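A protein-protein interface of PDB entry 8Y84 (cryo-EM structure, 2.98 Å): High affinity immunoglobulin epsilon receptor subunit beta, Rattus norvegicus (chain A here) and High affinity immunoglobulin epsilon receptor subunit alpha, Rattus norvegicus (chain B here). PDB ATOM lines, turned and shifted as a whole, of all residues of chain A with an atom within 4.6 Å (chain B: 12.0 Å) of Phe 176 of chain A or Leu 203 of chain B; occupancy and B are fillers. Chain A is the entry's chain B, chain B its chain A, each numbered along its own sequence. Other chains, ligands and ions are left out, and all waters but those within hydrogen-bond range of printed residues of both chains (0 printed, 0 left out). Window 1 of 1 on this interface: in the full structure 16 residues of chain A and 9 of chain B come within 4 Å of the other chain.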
ATOM      1  N   THR A  82     -25.626 -12.502 -11.991  1.00  0.00           N
ATOM      2  CA  THR A  82     -25.212 -13.684 -12.740  1.00  0.00           C
ATOM      3  C   THR A  82     -26.048 -13.900 -13.996  1.00  0.00           C
ATOM      4  O   THR A  82     -25.510 -14.287 -15.037  1.00  0.00           O
ATOM      5  CB  THR A  82     -25.278 -14.920 -11.847  1.00  0.00           C
ATOM      6  OG1 THR A  82     -26.640 -15.188 -11.499  1.00  0.00           O
ATOM      7  CG2 THR A  82     -24.468 -14.702 -10.580  1.00  0.00           C
ATOM      8  N   LEU A  83     -27.354 -13.664 -13.925  1.00  0.00           N
ATOM      9  CA  LEU A  83     -28.223 -13.936 -15.060  1.00  0.00           C
ATOM     10  C   LEU A  83     -28.184 -12.799 -16.068  1.00  0.00           C
ATOM     11  O   LEU A  83     -28.205 -11.621 -15.703  1.00  0.00           O
ATOM     12  CB  LEU A  83     -29.662 -14.159 -14.599  1.00  0.00           C
ATOM     13  CG  LEU A  83     -30.045 -15.570 -14.164  1.00  0.00           C
ATOM     14  CD1 LEU A  83     -31.530 -15.653 -13.885  1.00  0.00           C
ATOM     15  CD2 LEU A  83     -29.650 -16.571 -15.220  1.00  0.00           C
ATOM     16  N   PHE A 172     -33.181 -24.838 -18.087  1.00  0.00           N
ATOM     17  CA  PHE A 172     -32.429 -24.921 -16.838  1.00  0.00           C
ATOM     18  C   PHE A 172     -32.588 -23.665 -16.000  1.00  0.00           C
ATOM     19  O   PHE A 172     -32.716 -23.749 -14.776  1.00  0.00           O
ATOM     20  CB  PHE A 172     -30.954 -25.171 -17.117  1.00  0.00           C
ATOM     21  CG  PHE A 172     -30.178 -25.587 -15.905  1.00  0.00           C
ATOM     22  CD1 PHE A 172     -30.121 -26.917 -15.538  1.00  0.00           C
ATOM     23  CD2 PHE A 172     -29.496 -24.655 -15.140  1.00  0.00           C
ATOM     24  CE1 PHE A 172     -29.412 -27.310 -14.434  1.00  0.00           C
ATOM     25  CE2 PHE A 172     -28.793 -25.046 -14.031  1.00  0.00           C
ATOM     26  CZ  PHE A 172     -28.746 -26.377 -13.686  1.00  0.00           C
ATOM     27  N   VAL A 173     -32.555 -22.491 -16.632  1.00  0.00           N
ATOM     28  CA  VAL A 173     -32.719 -21.254 -15.877  1.00  0.00           C
ATOM     29  C   VAL A 173     -34.153 -21.122 -15.371  1.00  0.00           C
ATOM     30  O   VAL A 173     -34.378 -20.638 -14.258  1.00  0.00           O
ATOM     31  CB  VAL A 173     -32.255 -20.068 -16.743  1.00  0.00           C
ATOM     32  CG1 VAL A 173     -32.663 -18.732 -16.163  1.00  0.00           C
ATOM     33  CG2 VAL A 173     -30.754 -20.118 -16.871  1.00  0.00           C
ATOM     34  N   THR A 174     -35.134 -21.617 -16.129  1.00  0.00           N
ATOM     35  CA  THR A 174     -36.512 -21.648 -15.653  1.00  0.00           C
ATOM     36  C   THR A 174     -36.684 -22.603 -14.479  1.00  0.00           C
ATOM     37  O   THR A 174     -37.411 -22.295 -13.534  1.00  0.00           O
ATOM     38  CB  THR A 174     -37.441 -22.031 -16.797  1.00  0.00           C
ATOM     39  OG1 THR A 174     -37.115 -21.240 -17.945  1.00  0.00           O
ATOM     40  CG2 THR A 174     -38.888 -21.791 -16.422  1.00  0.00           C
ATOM     41  N   SER A 175     -36.008 -23.755 -14.503  1.00  0.00           N
ATOM     42  CA  SER A 175     -36.080 -24.674 -13.369  1.00  0.00           C
ATOM     43  C   SER A 175     -35.358 -24.123 -12.145  1.00  0.00           C
ATOM     44  O   SER A 175     -35.802 -24.328 -11.011  1.00  0.00           O
ATOM     45  CB  SER A 175     -35.483 -26.016 -13.751  1.00  0.00           C
ATOM     46  OG  SER A 175     -34.089 -25.979 -13.532  1.00  0.00           O
ATOM     47  N   PHE A 176     -34.230 -23.441 -12.356  1.00  0.00           N
ATOM     48  CA  PHE A 176     -33.515 -22.796 -11.259  1.00  0.00           C
ATOM     49  C   PHE A 176     -34.349 -21.681 -10.644  1.00  0.00           C
ATOM     50  O   PHE A 176     -34.410 -21.540  -9.417  1.00  0.00           O
ATOM     51  CB  PHE A 176     -32.173 -22.265 -11.769  1.00  0.00           C
ATOM     52  CG  PHE A 176     -31.600 -21.150 -10.950  1.00  0.00           C
ATOM     53  CD1 PHE A 176     -31.037 -21.405  -9.717  1.00  0.00           C
ATOM     54  CD2 PHE A 176     -31.601 -19.848 -11.423  1.00  0.00           C
ATOM     55  CE1 PHE A 176     -30.505 -20.387  -8.956  1.00  0.00           C
ATOM     56  CE2 PHE A 176     -31.071 -18.824 -10.667  1.00  0.00           C
ATOM     57  CZ  PHE A 176     -30.519 -19.096  -9.433  1.00  0.00           C
ATOM     58  N   ILE A 177     -35.018 -20.895 -11.487  1.00  0.00           N
ATOM     59  CA  ILE A 177     -35.921 -19.859 -11.007  1.00  0.00           C
ATOM     60  C   ILE A 177     -37.123 -20.485 -10.313  1.00  0.00           C
ATOM     61  O   ILE A 177     -37.597 -19.962  -9.312  1.00  0.00           O
ATOM     62  CB  ILE A 177     -36.316 -18.929 -12.172  1.00  0.00           C
ATOM     63  CG1 ILE A 177     -35.171 -17.973 -12.485  1.00  0.00           C
ATOM     64  CG2 ILE A 177     -37.543 -18.084 -11.873  1.00  0.00           C
ATOM     65  CD1 ILE A 177     -35.274 -17.362 -13.846  1.00  0.00           C
ATOM     66  N   THR A 178     -37.600 -21.638 -10.793  1.00  0.00           N
ATOM     67  CA  THR A 178     -38.706 -22.335 -10.134  1.00  0.00           C
ATOM     68  C   THR A 178     -38.319 -22.816  -8.743  1.00  0.00           C
ATOM     69  O   THR A 178     -39.104 -22.702  -7.798  1.00  0.00           O
ATOM     70  CB  THR A 178     -39.159 -23.515 -10.986  1.00  0.00           C
ATOM     71  OG1 THR A 178     -39.234 -23.112 -12.356  1.00  0.00           O
ATOM     72  CG2 THR A 178     -40.512 -24.013 -10.537  1.00  0.00           C
ATOM     73  N   GLU A 179     -37.098 -23.332  -8.600  1.00  0.00           N
ATOM     74  CA  GLU A 179     -36.584 -23.724  -7.292  1.00  0.00           C
ATOM     75  C   GLU A 179     -36.428 -22.517  -6.370  1.00  0.00           C
ATOM     76  O   GLU A 179     -36.776 -22.575  -5.182  1.00  0.00           O
ATOM     77  CB  GLU A 179     -35.251 -24.445  -7.480  1.00  0.00           C
ATOM     78  CG  GLU A 179     -34.579 -24.889  -6.218  1.00  0.00           C
ATOM     79  CD  GLU A 179     -33.385 -25.781  -6.482  1.00  0.00           C
ATOM     80  OE1 GLU A 179     -32.674 -26.129  -5.518  1.00  0.00           O
ATOM     81  OE2 GLU A 179     -33.156 -26.134  -7.657  1.00  0.00           O
ATOM     82  N   LEU A 180     -35.940 -21.402  -6.914  1.00  0.00           N
ATOM     83  CA  LEU A 180     -35.748 -20.194  -6.121  1.00  0.00           C
ATOM     84  C   LEU A 180     -37.079 -19.528  -5.770  1.00  0.00           C
ATOM     85  O   LEU A 180     -37.218 -18.966  -4.685  1.00  0.00           O
ATOM     86  CB  LEU A 180     -34.810 -19.259  -6.886  1.00  0.00           C
ATOM     87  CG  LEU A 180     -34.184 -17.995  -6.313  1.00  0.00           C
ATOM     88  CD1 LEU A 180     -32.832 -17.809  -6.946  1.00  0.00           C
ATOM     89  CD2 LEU A 180     -35.025 -16.803  -6.635  1.00  0.00           C
ATOM     90  N   ILE B 198     -24.702 -26.243 -21.009  1.00  0.00           N
ATOM     91  CA  ILE B 198     -25.586 -25.080 -20.966  1.00  0.00           C
ATOM     92  C   ILE B 198     -24.832 -23.773 -20.667  1.00  0.00           C
ATOM     93  O   ILE B 198     -25.332 -22.728 -21.037  1.00  0.00           O
ATOM     94  CB  ILE B 198     -26.715 -25.315 -19.966  1.00  0.00           C
ATOM     95  CG1 ILE B 198     -26.151 -25.763 -18.631  1.00  0.00           C
ATOM     96  CG2 ILE B 198     -27.674 -26.379 -20.496  1.00  0.00           C
ATOM     97  CD1 ILE B 198     -27.216 -26.057 -17.643  1.00  0.00           C
ATOM     98  N   GLU B 199     -23.742 -23.691 -19.843  1.00  0.00           N
ATOM     99  CA  GLU B 199     -23.180 -22.414 -19.217  1.00  0.00           C
ATOM    100  C   GLU B 199     -24.203 -21.647 -18.382  1.00  0.00           C
ATOM    101  O   GLU B 199     -24.281 -20.423 -18.465  1.00  0.00           O
ATOM    102  CB  GLU B 199     -22.532 -21.434 -20.225  1.00  0.00           C
ATOM    103  CG  GLU B 199     -21.236 -21.905 -20.869  1.00  0.00           C
ATOM    104  CD  GLU B 199     -21.455 -22.559 -22.215  1.00  0.00           C
ATOM    105  OE1 GLU B 199     -22.599 -22.526 -22.715  1.00  0.00           O
ATOM    106  OE2 GLU B 199     -20.481 -23.102 -22.776  1.00  0.00           O
ATOM    107  N   TYR B 200     -25.015 -22.357 -17.597  1.00  0.00           N
ATOM    108  CA  TYR B 200     -25.651 -21.755 -16.427  1.00  0.00           C
ATOM    109  C   TYR B 200     -25.772 -22.747 -15.278  1.00  0.00           C
ATOM    110  O   TYR B 200     -26.693 -22.640 -14.464  1.00  0.00           O
ATOM    111  CB  TYR B 200     -27.019 -21.150 -16.755  1.00  0.00           C
ATOM    112  CG  TYR B 200     -26.950 -19.684 -17.132  1.00  0.00           C
ATOM    113  CD1 TYR B 200     -27.421 -19.229 -18.353  1.00  0.00           C
ATOM    114  CD2 TYR B 200     -26.415 -18.754 -16.254  1.00  0.00           C
ATOM    115  CE1 TYR B 200     -27.350 -17.897 -18.693  1.00  0.00           C
ATOM    116  CE2 TYR B 200     -26.346 -17.417 -16.584  1.00  0.00           C
ATOM    117  CZ  TYR B 200     -26.816 -16.996 -17.803  1.00  0.00           C
ATOM    118  OH  TYR B 200     -26.748 -15.664 -18.139  1.00  0.00           O
ATOM    119  N   ARG B 201     -24.850 -23.709 -15.197  1.00  0.00           N
ATOM    120  CA  ARG B 201     -24.911 -24.728 -14.155  1.00  0.00           C
ATOM    121  C   ARG B 201     -24.615 -24.159 -12.774  1.00  0.00           C
ATOM    122  O   ARG B 201     -25.181 -24.632 -11.778  1.00  0.00           O
ATOM    123  CB  ARG B 201     -23.924 -25.852 -14.463  1.00  0.00           C
ATOM    124  CG  ARG B 201     -24.430 -26.890 -15.428  1.00  0.00           C
ATOM    125  CD  ARG B 201     -25.439 -27.811 -14.776  1.00  0.00           C
ATOM    126  NE  ARG B 201     -26.062 -28.697 -15.753  1.00  0.00           N
ATOM    127  CZ  ARG B 201     -25.563 -29.871 -16.123  1.00  0.00           C
ATOM    128  NH1 ARG B 201     -26.198 -30.610 -17.020  1.00  0.00           N
ATOM    129  NH2 ARG B 201     -24.431 -30.308 -15.593  1.00  0.00           N
ATOM    130  N   TRP B 202     -23.762 -23.129 -12.696  1.00  0.00           N
ATOM    131  CA  TRP B 202     -23.304 -22.603 -11.413  1.00  0.00           C
ATOM    132  C   TRP B 202     -24.414 -21.946 -10.606  1.00  0.00           C
ATOM    133  O   TRP B 202     -24.217 -21.685  -9.414  1.00  0.00           O
ATOM    134  CB  TRP B 202     -22.168 -21.595 -11.618  1.00  0.00           C
ATOM    135  CG  TRP B 202     -22.600 -20.265 -12.177  1.00  0.00           C
ATOM    136  CD1 TRP B 202     -23.010 -19.162 -11.478  1.00  0.00           C
ATOM    137  CD2 TRP B 202     -22.634 -19.895 -13.554  1.00  0.00           C
ATOM    138  NE1 TRP B 202     -23.317 -18.143 -12.338  1.00  0.00           N
ATOM    139  CE2 TRP B 202     -23.089 -18.566 -13.620  1.00  0.00           C
ATOM    140  CE3 TRP B 202     -22.327 -20.562 -14.740  1.00  0.00           C
ATOM    141  CZ2 TRP B 202     -23.243 -17.892 -14.823  1.00  0.00           C
ATOM    142  CZ3 TRP B 202     -22.477 -19.893 -15.931  1.00  0.00           C
ATOM    143  CH2 TRP B 202     -22.932 -18.571 -15.967  1.00  0.00           C
ATOM    144  N   LEU B 203     -25.551 -21.638 -11.235  1.00  0.00           N
ATOM    145  CA  LEU B 203     -26.711 -21.155 -10.501  1.00  0.00           C
ATOM    146  C   LEU B 203     -27.194 -22.183  -9.492  1.00  0.00           C
ATOM    147  O   LEU B 203     -27.641 -21.817  -8.401  1.00  0.00           O
ATOM    148  CB  LEU B 203     -27.831 -20.803 -11.473  1.00  0.00           C
ATOM    149  CG  LEU B 203     -27.492 -19.849 -12.614  1.00  0.00           C
ATOM    150  CD1 LEU B 203     -28.633 -19.832 -13.603  1.00  0.00           C
ATOM    151  CD2 LEU B 203     -27.225 -18.457 -12.079  1.00  0.00           C
ATOM    152  N   GLN B 204     -27.073 -23.470  -9.808  1.00  0.00           N
ATOM    153  CA  GLN B 204     -27.412 -24.474  -8.814  1.00  0.00           C
ATOM    154  C   GLN B 204     -26.286 -24.715  -7.821  1.00  0.00           C
ATOM    155  O   GLN B 204     -26.458 -25.518  -6.900  1.00  0.00           O
ATOM    156  CB  GLN B 204     -27.816 -25.780  -9.492  1.00  0.00           C
ATOM    157  CG  GLN B 204     -29.132 -25.671 -10.237  1.00  0.00           C
ATOM    158  CD  GLN B 204     -30.338 -25.940  -9.363  1.00  0.00           C
ATOM    159  OE1 GLN B 204     -30.215 -26.133  -8.155  1.00  0.00           O
ATOM    160  NE2 GLN B 204     -31.518 -25.950  -9.972  1.00  0.00           N
ATOM    161  N   LEU B 205     -25.144 -24.055  -7.994  1.00  0.00           N
ATOM    162  CA  LEU B 205     -24.165 -23.898  -6.931  1.00  0.00           C
ATOM    163  C   LEU B 205     -24.480 -22.707  -6.041  1.00  0.00           C
ATOM    164  O   LEU B 205     -23.760 -22.473  -5.068  1.00  0.00           O
ATOM    165  CB  LEU B 205     -22.760 -23.741  -7.513  1.00  0.00           C
ATOM    166  CG  LEU B 205     -22.050 -25.031  -7.920  1.00  0.00           C
ATOM    167  CD1 LEU B 205     -20.740 -24.709  -8.605  1.00  0.00           C
ATOM    168  CD2 LEU B 205     -21.823 -25.919  -6.713  1.00  0.00           C
ATOM    169  N   ILE B 206     -25.523 -21.941  -6.369  1.00  0.00           N
ATOM    170  CA  ILE B 206     -25.956 -20.851  -5.503  1.00  0.00           C
ATOM    171  C   ILE B 206     -26.581 -21.409  -4.231  1.00  0.00           C
ATOM    172  O   ILE B 206     -26.326 -20.914  -3.127  1.00  0.00           O
ATOM    173  CB  ILE B 206     -26.921 -19.926  -6.272  1.00  0.00           C
ATOM    174  CG1 ILE B 206     -26.158 -19.086  -7.306  1.00  0.00           C
ATOM    175  CG2 ILE B 206     -27.700 -19.013  -5.339  1.00  0.00           C
ATOM    176  CD1 ILE B 206     -24.953 -18.354  -6.757  1.00  0.00           C
ATOM    177  N   PHE B 207     -27.382 -22.475  -4.370  1.00  0.00           N
ATOM    178  CA  PHE B 207     -28.108 -23.033  -3.228  1.00  0.00           C
ATOM    179  C   PHE B 207     -27.217 -23.639  -2.141  1.00  0.00           C
ATOM    180  O   PHE B 207     -27.460 -23.344  -0.959  1.00  0.00           O
ATOM    181  CB  PHE B 207     -29.141 -24.048  -3.720  1.00  0.00           C
ATOM    182  CG  PHE B 207     -30.197 -23.449  -4.575  1.00  0.00           C
ATOM    183  CD1 PHE B 207     -30.184 -23.668  -5.938  1.00  0.00           C
ATOM    184  CD2 PHE B 207     -31.141 -22.592  -4.048  1.00  0.00           C
ATOM    185  CE1 PHE B 207     -31.138 -23.111  -6.748  1.00  0.00           C
ATOM    186  CE2 PHE B 207     -32.094 -22.012  -4.863  1.00  0.00           C
ATOM    187  CZ  PHE B 207     -32.091 -22.273  -6.213  1.00  0.00           C
ATOM    188  N   PRO B 208     -26.190 -24.512  -2.435  1.00  0.00           N
ATOM    189  CA  PRO B 208     -25.408 -25.042  -1.311  1.00  0.00           C
ATOM    190  C   PRO B 208     -24.444 -24.019  -0.739  1.00  0.00           C
ATOM    191  O   PRO B 208     -24.138 -24.066   0.457  1.00  0.00           O
ATOM    192  CB  PRO B 208     -24.665 -26.232  -1.924  1.00  0.00           C
ATOM    193  CG  PRO B 208     -24.501 -25.890  -3.312  1.00  0.00           C
ATOM    194  CD  PRO B 208     -25.699 -25.095  -3.703  1.00  0.00           C
ATOM    195  N   SER B 209     -23.971 -23.095  -1.584  1.00  0.00           N
ATOM    196  CA  SER B 209     -23.131 -22.002  -1.106  1.00  0.00           C
ATOM    197  C   SER B 209     -23.892 -21.127  -0.126  1.00  0.00           C
ATOM    198  O   SER B 209     -23.383 -20.808   0.953  1.00  0.00           O
ATOM    199  CB  SER B 209     -22.625 -21.170  -2.278  1.00  0.00           C
ATOM    200  OG  SER B 209     -21.817 -20.100  -1.818  1.00  0.00           O
ATOM    201  N   LEU B 210     -25.145 -20.803  -0.447  1.00  0.00           N
ATOM    202  CA  LEU B 210     -26.000 -20.114   0.507  1.00  0.00           C
ATOM    203  C   LEU B 210     -26.320 -20.983   1.714  1.00  0.00           C
ATOM    204  O   LEU B 210     -26.637 -20.450   2.778  1.00  0.00           O
ATOM    205  CB  LEU B 210     -27.290 -19.657  -0.171  1.00  0.00           C
ATOM    206  CG  LEU B 210     -27.971 -18.474   0.515  1.00  0.00           C
ATOM    207  CD1 LEU B 210     -26.985 -17.336   0.670  1.00  0.00           C
ATOM    208  CD2 LEU B 210     -29.187 -18.028  -0.254  1.00  0.00           C
ATOM    209  N   ALA B 211     -26.226 -22.305   1.578  1.00  0.00           N
ATOM    210  CA  ALA B 211     -26.241 -23.151   2.758  1.00  0.00           C
ATOM    211  C   ALA B 211     -24.969 -22.997   3.578  1.00  0.00           C
ATOM    212  O   ALA B 211     -25.048 -22.815   4.799  1.00  0.00           O
ATOM    213  CB  ALA B 211     -26.430 -24.606   2.356  1.00  0.00           C
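Thr 82 of chain A touches just these residues of chain B: Tyr 200 (3.6 Å), Trp 202 (3.8 Å) and Leu 203 (3.4 Å). Leu 83 of chain A touches just these residues of chain B: Tyr 200 and Leu 203. Val 173 of chain A touches just these residues of chain B: Tyr 200 and Leu 203. Phe 176 of chain A touches just these residues of chain B: Leu 203, Gln 204 and Phe 207. No residue of chain B comes within 4 Å of Ile 177 of chain A. Glu 179 of chain A touches just these residues of chain B: Gln 204 and Phe 207. Of the printed residues of chain A, Ile 198 of chain B touches Phe 172 (3.5 Å). Of the printed residues of chain A, Tyr 200 of chain B touches Thr 82 (3.6 Å), Leu 83 (3.7 Å), Phe 172 (3.2 Å) and Val 173 (3.8 Å). Printed residues of chain A within 4 Å of Arg 201 of chain B: Phe 172 (3.8 Å). Leu 203 of chain B touches just these residues of chain A: Thr 82 (3.4 Å), Leu 83 (3.8 Å), Val 173 (3.9 Å) and Phe 176 (3.2 Å). Printed residues of chain A within 4 Å of Gln 204 of chain B: Phe 172, Phe 176 and Glu 179. Printed residues of chain A within 4 Å of Phe 207 of chain B: Phe 176 (3.4 Å) and Glu 179 (3.5 Å).
Hydrophobic or aromatic side chains of chain B within 4 Å of the printed part of chain A: Ile 198, Tyr 200, Trp 202, Leu 203 and Phe 207. Of the 11 printed residues of chain A, 6 touch a printed residue of chain B. Printed residues of chain A that touch a printed residue of chain B: Thr 82, Leu 83, Phe 172, Val 173, Phe 176 and Glu 179. Hydrophobic or aromatic side chains of chain A within 4 Å of the printed part of chain B: Leu 83, Phe 172, Val 173 and Phe 176.
Among the printed residues, pairs that only touch across the chains: Phe 172 of chain A with Tyr 200 of chain B (3.2 Å), Phe 176 of chain A with Leu 203 of chain B (3.2 Å), Thr 82 of chain A with Leu 203 of chain B (3.4 Å), Phe 176 of chain A with Phe 207 of chain B (3.4 Å), Phe 172 of chain A with Ile 198 of chain B (3.5 Å), Glu 179 of chain A with Phe 207 of chain B (3.5 Å), Phe 172 of chain A with Gln 204 of chain B (3.5 Å), Thr 82 of chain A with Tyr 200 of chain B (3.6 Å), Leu 83 of chain A with Tyr 200 of chain B (3.7 Å), Val 173 of chain A with Tyr 200 of chain B (3.8 Å), Phe 172 of chain A with Arg 201 of chain B (3.8 Å), Leu 83 of chain A with Leu 203 of chain B (3.8 Å), Thr 82 of chain A with Trp 202 of chain B (3.8 Å), Val 173 of chain A with Leu 203 of chain B (3.9 Å) and Phe 176 of chain A with Gln 204 of chain B (3.9 Å).
OE2 of Glu 179 of chain A is in hydrogen-bond range of NE2 of Gln 204 of chain B.
The backbone carbonyl oxygen of Phe 172 of chain A sits at hydrogen-bond distance from the side-chain hydroxyl of Ser 175 of chain A, 2.9 Å away.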
